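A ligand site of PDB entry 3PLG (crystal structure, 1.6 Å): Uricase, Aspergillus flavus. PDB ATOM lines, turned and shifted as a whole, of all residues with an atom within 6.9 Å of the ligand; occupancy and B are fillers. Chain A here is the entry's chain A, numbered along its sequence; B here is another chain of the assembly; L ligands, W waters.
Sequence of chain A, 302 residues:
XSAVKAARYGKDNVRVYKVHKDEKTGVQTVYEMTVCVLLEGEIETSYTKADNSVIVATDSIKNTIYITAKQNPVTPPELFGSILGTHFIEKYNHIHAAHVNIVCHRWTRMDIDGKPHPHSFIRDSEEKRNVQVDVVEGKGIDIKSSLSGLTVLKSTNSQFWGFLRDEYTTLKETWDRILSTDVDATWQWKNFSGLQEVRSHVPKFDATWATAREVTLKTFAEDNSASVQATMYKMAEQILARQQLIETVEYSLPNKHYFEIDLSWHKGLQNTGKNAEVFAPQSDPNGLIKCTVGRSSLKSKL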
ATOM      1  N   SER A 158       3.262  23.173  -9.350  1.00  0.00           N
ATOM      2  CA  SER A 158       3.713  23.375  -7.985  1.00  0.00           C
ATOM      3  C   SER A 158       5.236  23.248  -8.011  1.00  0.00           C
ATOM      4  O   SER A 158       5.796  22.360  -8.654  1.00  0.00           O
ATOM      5  CB  SER A 158       3.113  22.308  -7.058  1.00  0.00           C
ATOM      6  OG  SER A 158       3.693  22.379  -5.758  1.00  0.00           O
ATOM      7  N   GLN A 159       5.899  24.158  -7.297  1.00  0.00           N
ATOM      8  CA  GLN A 159       7.348  24.207  -7.236  1.00  0.00           C
ATOM      9  C   GLN A 159       7.776  24.339  -5.786  1.00  0.00           C
ATOM     10  O   GLN A 159       6.991  24.783  -4.923  1.00  0.00           O
ATOM     11  CB  GLN A 159       7.888  25.456  -8.001  1.00  0.00           C
ATOM     12  CG  GLN A 159       7.359  25.555  -9.417  1.00  0.00           C
ATOM     13  CD  GLN A 159       7.959  26.699 -10.224  1.00  0.00           C
ATOM     14  OE1 GLN A 159       8.784  27.469  -9.734  1.00  0.00           O
ATOM     15  NE2 GLN A 159       7.544  26.795 -11.472  1.00  0.00           N
ATOM     16  N   PHE A 160       9.007  23.958  -5.512  1.00  0.00           N
ATOM     17  CA  PHE A 160       9.598  24.236  -4.223  1.00  0.00           C
ATOM     18  C   PHE A 160      11.109  24.276  -4.311  1.00  0.00           C
ATOM     19  O   PHE A 160      11.778  23.254  -4.343  1.00  0.00           O
ATOM     20  CB  PHE A 160       9.083  23.256  -3.138  1.00  0.00           C
ATOM     21  CG  PHE A 160       9.435  23.697  -1.736  1.00  0.00           C
ATOM     22  CD1 PHE A 160       8.929  24.892  -1.218  1.00  0.00           C
ATOM     23  CD2 PHE A 160      10.318  22.944  -0.938  1.00  0.00           C
ATOM     24  CE1 PHE A 160       9.284  25.327   0.053  1.00  0.00           C
ATOM     25  CE2 PHE A 160      10.663  23.370   0.333  1.00  0.00           C
ATOM     26  CZ  PHE A 160      10.157  24.575   0.831  1.00  0.00           C
ATOM     27  N   PHE A 163      14.832  27.092  -0.705  1.00  0.00           N
ATOM     28  CA  PHE A 163      14.789  26.970   0.744  1.00  0.00           C
ATOM     29  C   PHE A 163      16.193  26.848   1.370  1.00  0.00           C
ATOM     30  O   PHE A 163      17.178  26.640   0.659  1.00  0.00           O
ATOM     31  CB  PHE A 163      13.922  25.765   1.156  1.00  0.00           C
ATOM     32  CG  PHE A 163      14.277  24.505   0.412  1.00  0.00           C
ATOM     33  CD1 PHE A 163      13.646  24.189  -0.779  1.00  0.00           C
ATOM     34  CD2 PHE A 163      15.226  23.617   0.947  1.00  0.00           C
ATOM     35  CE1 PHE A 163      13.959  23.012  -1.466  1.00  0.00           C
ATOM     36  CE2 PHE A 163      15.539  22.440   0.260  1.00  0.00           C
ATOM     37  CZ  PHE A 163      14.926  22.147  -0.939  1.00  0.00           C
ATOM     38  N   LEU A 171      16.792  17.314   0.854  1.00  0.00           N
ATOM     39  CA  LEU A 171      15.737  17.567  -0.123  1.00  0.00           C
ATOM     40  C   LEU A 171      16.254  18.291  -1.358  1.00  0.00           C
ATOM     41  O   LEU A 171      16.912  19.332  -1.245  1.00  0.00           O
ATOM     42  CB  LEU A 171      14.631  18.423   0.535  1.00  0.00           C
ATOM     43  CG  LEU A 171      13.393  18.729  -0.333  1.00  0.00           C
ATOM     44  CD1 LEU A 171      12.603  17.448  -0.644  1.00  0.00           C
ATOM     45  CD2 LEU A 171      12.504  19.734   0.391  1.00  0.00           C
ATOM     46  N   ARG A 177       6.261  19.504  -9.170  1.00  0.00           N
ATOM     47  CA  ARG A 177       5.919  18.406  -8.240  1.00  0.00           C
ATOM     48  C   ARG A 177       4.408  18.289  -8.134  1.00  0.00           C
ATOM     49  O   ARG A 177       3.661  19.169  -8.548  1.00  0.00           O
ATOM     50  CB  ARG A 177       6.524  18.645  -6.854  1.00  0.00           C
ATOM     51  CG  ARG A 177       5.937  19.862  -6.158  1.00  0.00           C
ATOM     52  CD  ARG A 177       6.543  20.088  -4.793  1.00  0.00           C
ATOM     53  NE  ARG A 177       5.821  21.169  -4.108  1.00  0.00           N
ATOM     54  CZ  ARG A 177       5.976  21.502  -2.822  1.00  0.00           C
ATOM     55  NH1 ARG A 177       6.862  20.866  -2.058  1.00  0.00           N
ATOM     56  NH2 ARG A 177       5.261  22.506  -2.311  1.00  0.00           N
ATOM     57  N   LEU A 179       1.130  18.400  -5.757  1.00  0.00           N
ATOM     58  CA  LEU A 179       0.727  19.042  -4.504  1.00  0.00           C
ATOM     59  C   LEU A 179      -0.667  18.527  -4.133  1.00  0.00           C
ATOM     60  O   LEU A 179      -1.602  18.607  -4.917  1.00  0.00           O
ATOM     61  CB  LEU A 179       0.715  20.567  -4.670  1.00  0.00           C
ATOM     62  CG  LEU A 179       0.345  21.389  -3.430  1.00  0.00           C
ATOM     63  CD1 LEU A 179       1.328  21.136  -2.305  1.00  0.00           C
ATOM     64  CD2 LEU A 179       0.340  22.893  -3.790  1.00  0.00           C
ATOM     65  N   SER A 225       2.279  27.451  -7.864  1.00  0.00           N
ATOM     66  CA  SER A 225       2.546  27.554  -6.452  1.00  0.00           C
ATOM     67  C   SER A 225       4.031  27.530  -6.136  1.00  0.00           C
ATOM     68  O   SER A 225       4.746  26.603  -6.526  1.00  0.00           O
ATOM     69  CB  SER A 225       1.826  26.397  -5.732  1.00  0.00           C
ATOM     70  OG  SER A 225       2.166  26.391  -4.382  1.00  0.00           O
ATOM     71  N   ALA A 226       4.495  28.512  -5.369  1.00  0.00           N
ATOM     72  CA  ALA A 226       5.882  28.605  -4.949  1.00  0.00           C
ATOM     73  C   ALA A 226       6.145  27.812  -3.689  1.00  0.00           C
ATOM     74  O   ALA A 226       7.303  27.519  -3.354  1.00  0.00           O
ATOM     75  CB  ALA A 226       6.269  30.077  -4.728  1.00  0.00           C
ATOM     76  N   SER A 227       5.057  27.508  -2.971  1.00  0.00           N
ATOM     77  CA  SER A 227       5.107  26.748  -1.712  1.00  0.00           C
ATOM     78  C   SER A 227       3.685  26.672  -1.211  1.00  0.00           C
ATOM     79  O   SER A 227       2.825  27.434  -1.638  1.00  0.00           O
ATOM     80  CB  SER A 227       5.957  27.451  -0.645  1.00  0.00           C
ATOM     81  OG  SER A 227       5.364  28.694  -0.258  1.00  0.00           O
ATOM     82  N   VAL A 228       3.435  25.794  -0.237  1.00  0.00           N
ATOM     83  CA  VAL A 228       2.107  25.762   0.368  1.00  0.00           C
ATOM     84  C   VAL A 228       1.844  27.109   1.054  1.00  0.00           C
ATOM     85  O   VAL A 228       0.737  27.662   0.957  1.00  0.00           O
ATOM     86  CB  VAL A 228       2.024  24.576   1.371  1.00  0.00           C
ATOM     87  CG1 VAL A 228       0.730  24.625   2.145  1.00  0.00           C
ATOM     88  CG2 VAL A 228       2.113  23.269   0.581  1.00  0.00           C
ATOM     89  N   GLN A 229       2.861  27.610   1.744  1.00  0.00           N
ATOM     90  CA  GLN A 229       2.802  28.892   2.480  1.00  0.00           C
ATOM     91  C   GLN A 229       2.300  30.004   1.549  1.00  0.00           C
ATOM     92  O   GLN A 229       1.359  30.759   1.877  1.00  0.00           O
ATOM     93  CB  GLN A 229       4.201  29.257   2.963  1.00  0.00           C
ATOM     94  CG  GLN A 229       4.710  28.425   4.178  1.00  0.00           C
ATOM     95  CD  GLN A 229       5.427  27.135   3.816  1.00  0.00           C
ATOM     96  OE1 GLN A 229       5.199  26.540   2.754  1.00  0.00           O
ATOM     97  NE2 GLN A 229       6.294  26.687   4.736  1.00  0.00           N
ATOM     98  N   ALA A 230       2.906  30.119   0.370  1.00  0.00           N
ATOM     99  CA  ALA A 230       2.557  31.236  -0.495  1.00  0.00           C
ATOM    100  C   ALA A 230       1.140  31.110  -1.070  1.00  0.00           C
ATOM    101  O   ALA A 230       0.391  32.094  -1.184  1.00  0.00           O
ATOM    102  CB  ALA A 230       3.590  31.383  -1.592  1.00  0.00           C
ATOM    103  N   ASN A 255       0.863  18.655   3.915  1.00  0.00           N
ATOM    104  CA  ASN A 255       1.466  18.509   2.623  1.00  0.00           C
ATOM    105  C   ASN A 255       1.586  16.985   2.460  1.00  0.00           C
ATOM    106  O   ASN A 255       2.417  16.370   3.112  1.00  0.00           O
ATOM    107  CB  ASN A 255       2.806  19.257   2.591  1.00  0.00           C
ATOM    108  CG  ASN A 255       3.417  19.310   1.210  1.00  0.00           C
ATOM    109  OD1 ASN A 255       2.814  18.842   0.231  1.00  0.00           O
ATOM    110  ND2 ASN A 255       4.628  19.870   1.107  1.00  0.00           N
ATOM    111  N   HIS A 257       2.655  13.918   0.741  1.00  0.00           N
ATOM    112  CA  HIS A 257       3.717  13.737  -0.246  1.00  0.00           C
ATOM    113  C   HIS A 257       3.519  12.548  -1.165  1.00  0.00           C
ATOM    114  O   HIS A 257       3.078  11.474  -0.737  1.00  0.00           O
ATOM    115  CB  HIS A 257       5.062  13.598   0.463  1.00  0.00           C
ATOM    116  CG  HIS A 257       5.333  14.678   1.458  1.00  0.00           C
ATOM    117  ND1 HIS A 257       5.603  15.976   1.082  1.00  0.00           N
ATOM    118  CD2 HIS A 257       5.353  14.667   2.814  1.00  0.00           C
ATOM    119  CE1 HIS A 257       5.804  16.713   2.165  1.00  0.00           C
ATOM    120  NE2 HIS A 257       5.650  15.941   3.229  1.00  0.00           N
ATOM    121  N   GLY A 287       4.144  17.080   5.886  1.00  0.00           N
ATOM    122  CA  GLY A 287       4.287  18.482   6.263  1.00  0.00           C
ATOM    123  C   GLY A 287       2.972  18.993   6.837  1.00  0.00           C
ATOM    124  O   GLY A 287       1.909  18.473   6.536  1.00  0.00           O
ATOM    125  N   ILE A 289       1.357  22.884   7.632  1.00  0.00           N
ATOM    126  CA  ILE A 289       1.612  24.311   7.439  1.00  0.00           C
ATOM    127  C   ILE A 289       0.383  25.058   7.881  1.00  0.00           C
ATOM    128  O   ILE A 289      -0.731  24.729   7.439  1.00  0.00           O
ATOM    129  CB  ILE A 289       1.887  24.639   5.932  1.00  0.00           C
ATOM    130  CG1 ILE A 289       2.863  23.620   5.270  1.00  0.00           C
ATOM    131  CG2 ILE A 289       2.398  26.082   5.809  1.00  0.00           C
ATOM    132  CD1 ILE A 289       4.145  23.446   5.915  1.00  0.00           C
ATOM    133  N   TYR B   9       4.816  25.979  11.191  1.00  0.00           N
ATOM    134  CA  TYR B   9       4.846  24.958  10.156  1.00  0.00           C
ATOM    135  C   TYR B   9       5.900  23.922  10.579  1.00  0.00           C
ATOM    136  O   TYR B   9       6.793  24.198  11.389  1.00  0.00           O
ATOM    137  CB  TYR B   9       5.185  25.562   8.776  1.00  0.00           C
ATOM    138  CG  TYR B   9       6.678  25.733   8.611  1.00  0.00           C
ATOM    139  CD1 TYR B   9       7.366  26.711   9.314  1.00  0.00           C
ATOM    140  CD2 TYR B   9       7.409  24.838   7.841  1.00  0.00           C
ATOM    141  CE1 TYR B   9       8.757  26.816   9.235  1.00  0.00           C
ATOM    142  CE2 TYR B   9       8.789  24.935   7.738  1.00  0.00           C
ATOM    143  CZ  TYR B   9       9.459  25.935   8.450  1.00  0.00           C
ATOM    144  OH  TYR B   9      10.829  26.022   8.372  1.00  0.00           O
ATOM    145  N   GLY B  10       5.794  22.717  10.033  1.00  0.00           N
ATOM    146  CA  GLY B  10       6.767  21.700  10.381  1.00  0.00           C
ATOM    147  C   GLY B  10       6.360  20.346   9.849  1.00  0.00           C
ATOM    148  O   GLY B  10       5.710  20.241   8.815  1.00  0.00           O
ATOM    149  N   LYS B  11       6.731  19.300  10.580  1.00  0.00           N
ATOM    150  CA  LYS B  11       6.491  17.926  10.117  1.00  0.00           C
ATOM    151  C   LYS B  11       5.696  17.201  11.188  1.00  0.00           C
ATOM    152  O   LYS B  11       6.013  17.297  12.382  1.00  0.00           O
ATOM    153  CB  LYS B  11       7.817  17.188   9.897  1.00  0.00           C
ATOM    154  CG  LYS B  11       7.715  15.974   8.992  1.00  0.00           C
ATOM    155  CD  LYS B  11       7.290  16.364   7.580  1.00  0.00           C
ATOM    156  CE  LYS B  11       8.176  15.765   6.526  1.00  0.00           C
ATOM    157  NZ  LYS B  11       7.977  16.471   5.209  1.00  0.00           N
ATOM    158  N   ASN B  52      11.399  31.698   0.001  1.00  0.00           N
ATOM    159  CA  ASN B  52      11.682  30.416   0.652  1.00  0.00           C
ATOM    160  C   ASN B  52      12.988  30.391   1.447  1.00  0.00           C
ATOM    161  O   ASN B  52      13.297  29.395   2.100  1.00  0.00           O
ATOM    162  CB  ASN B  52      11.592  29.254  -0.342  1.00  0.00           C
ATOM    163  CG  ASN B  52      10.171  29.024  -0.838  1.00  0.00           C
ATOM    164  OD1 ASN B  52       9.211  29.389  -0.160  1.00  0.00           O
ATOM    165  ND2 ASN B  52      10.020  28.424  -2.017  1.00  0.00           N
ATOM    166  N   ILE B  55      12.821  29.341   5.050  1.00  0.00           N
ATOM    167  CA  ILE B  55      12.213  28.048   5.371  1.00  0.00           C
ATOM    168  C   ILE B  55      13.248  26.945   5.588  1.00  0.00           C
ATOM    169  O   ILE B  55      13.998  26.596   4.659  1.00  0.00           O
ATOM    170  CB  ILE B  55      11.224  27.575   4.281  1.00  0.00           C
ATOM    171  CG1 ILE B  55      10.036  28.530   4.154  1.00  0.00           C
ATOM    172  CG2 ILE B  55      10.665  26.148   4.650  1.00  0.00           C
ATOM    173  CD1 ILE B  55       9.169  28.230   2.889  1.00  0.00           C
ATOM    174  N   VAL B  56      13.273  26.423   6.808  1.00  0.00           N
ATOM    175  CA  VAL B  56      13.935  25.160   7.118  1.00  0.00           C
ATOM    176  C   VAL B  56      12.945  24.114   6.589  1.00  0.00           C
ATOM    177  O   VAL B  56      11.819  24.038   7.106  1.00  0.00           O
ATOM    178  CB  VAL B  56      14.180  25.027   8.631  1.00  0.00           C
ATOM    179  CG1 VAL B  56      14.764  23.637   8.956  1.00  0.00           C
ATOM    180  CG2 VAL B  56      15.117  26.136   9.122  1.00  0.00           C
ATOM    181  N   ALA B  57      13.317  23.368   5.543  1.00  0.00           N
ATOM    182  CA  ALA B  57      12.333  22.488   4.855  1.00  0.00           C
ATOM    183  C   ALA B  57      11.793  21.460   5.863  1.00  0.00           C
ATOM    184  O   ALA B  57      12.514  21.021   6.734  1.00  0.00           O
ATOM    185  CB  ALA B  57      12.957  21.782   3.619  1.00  0.00           C
ATOM    186  N   THR B  58      10.527  21.095   5.703  1.00  0.00           N
ATOM    187  CA  THR B  58       9.930  20.144   6.644  1.00  0.00           C
ATOM    188  C   THR B  58      10.691  18.804   6.532  1.00  0.00           C
ATOM    189  O   THR B  58      10.827  18.106   7.533  1.00  0.00           O
ATOM    190  CB  THR B  58       8.417  19.973   6.443  1.00  0.00           C
ATOM    191  OG1 THR B  58       8.177  19.356   5.172  1.00  0.00           O
ATOM    192  CG2 THR B  58       7.720  21.346   6.529  1.00  0.00           C
ATOM    193  N   ASP B  59      11.163  18.475   5.326  1.00  0.00           N
ATOM    194  CA  ASP B  59      11.984  17.271   5.138  1.00  0.00           C
ATOM    195  C   ASP B  59      13.229  17.297   6.018  1.00  0.00           C
ATOM    196  O   ASP B  59      13.640  16.279   6.557  1.00  0.00           O
ATOM    197  CB  ASP B  59      12.382  17.127   3.673  1.00  0.00           C
ATOM    198  CG  ASP B  59      12.990  15.779   3.381  1.00  0.00           C
ATOM    199  OD1 ASP B  59      12.217  14.798   3.285  1.00  0.00           O
ATOM    200  OD2 ASP B  59      14.237  15.705   3.245  1.00  0.00           O
ATOM    201  N   SER B  60      13.853  18.476   6.139  1.00  0.00           N
ATOM    202  CA  SER B  60      15.019  18.661   7.025  1.00  0.00           C
ATOM    203  C   SER B  60      14.665  18.502   8.494  1.00  0.00           C
ATOM    204  O   SER B  60      15.467  17.998   9.300  1.00  0.00           O
ATOM    205  CB  SER B  60      15.662  20.034   6.758  1.00  0.00           C
ATOM    206  OG  SER B  60      15.924  20.126   5.372  1.00  0.00           O
HETATM  207  N1  LIG L   1       6.581  24.010   2.109  1.00  0.00           N
HETATM  208  C1  LIG L   1       6.323  23.319   0.980  1.00  0.00           C
HETATM  209  O1  LIG L   1       5.448  23.744   0.202  1.00  0.00           O
HETATM  210  N2  LIG L   1       6.980  22.166   0.638  1.00  0.00           N
HETATM  211  C2  LIG L   1       7.942  21.713   1.457  1.00  0.00           C
HETATM  212  C3  LIG L   1       8.263  22.430   2.696  1.00  0.00           C
HETATM  213  C4  LIG L   1       7.511  23.663   3.005  1.00  0.00           C
HETATM  214  O2  LIG L   1       7.720  24.303   4.052  1.00  0.00           O
HETATM  215  N3  LIG L   1       9.266  21.787   3.333  1.00  0.00           N
HETATM  216  N4  LIG L   1       9.568  20.688   2.558  1.00  0.00           N
HETATM  217  N5  LIG L   1       8.774  20.641   1.415  1.00  0.00           N
HETATM  218  O   HOH W   1       5.863  20.022   3.702  1.00  0.00           O
HETATM  219  O   HOH W   2       8.576  18.568  -0.292  1.00  0.00           O
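Residues that only touch the ligand: Phe 160, Leu 171, Ser 227, Tyr 9 of chain B, Ile 55 of chain B, Ala 57 of chain B and Asp 59 of chain B. Hydrophobic or aromatic side chains that line the ligand: Phe 160, Leu 171, Val 228, Tyr 9 of chain B, Ile 55 of chain B and Ala 57 of chain B.
O of Asn 255 lies within hydrogen-bond range of NE2 of His 257 (3.3 Å). The side-chain hydroxyl (OH) of Tyr 9 of chain B sits at hydrogen-bond distance from the backbone carbonyl oxygen (O) of Val 56 of chain B (2.6 Å). OG1 of Thr 58 of chain B lies within hydrogen-bond range of NZ of Lys 11 of chain B, at 2.9 Å. The backbone NH (N) of Gln 229 sits close to the side-chain hydroxyl (OG) of Ser 227. N of Ala 230 sits at hydrogen-bond distance from OG of Ser 227, at 2.9 Å. O of Ser 227 is in hydrogen-bond range of OG of Ser 225, 3.0 Å away. N of Asn 255 lies within hydrogen-bond range of O of Gly 287. N of Arg 177 sits at hydrogen-bond distance from O of Ser 158, 2.9 Å away.
Water W2 lies within hydrogen-bond range of N5 of the ligand (2.7 Å) and NH1 of Arg 177 (3.4 Å). Water W1 bridges the side-chain hydroxyl (OG1) of Thr 58 of chain B and the side-chain amide nitrogen (ND2) of Asn 255.
NH2 of Arg 177 is in hydrogen-bond range of O1 of the ligand, 2.8 Å away. The backbone NH (N) of Val 228 lies within hydrogen-bond range of an oxygen (O1) of the ligand (2.9 Å). N3 of the ligand lies within hydrogen-bond range of OG1 of Thr 58 of chain B (3.2 Å). The backbone NH of Thr 58 of chain B is in hydrogen-bond range of a nitrogen (N3) of the ligand (2.8 Å). A nitrogen (N2) of the ligand sits close to the side-chain amide nitrogen (ND2) of Asn 255, 3.3 Å away. The side-chain amide nitrogen of Gln 229 is in hydrogen-bond range of an oxygen (O2) of the ligand.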
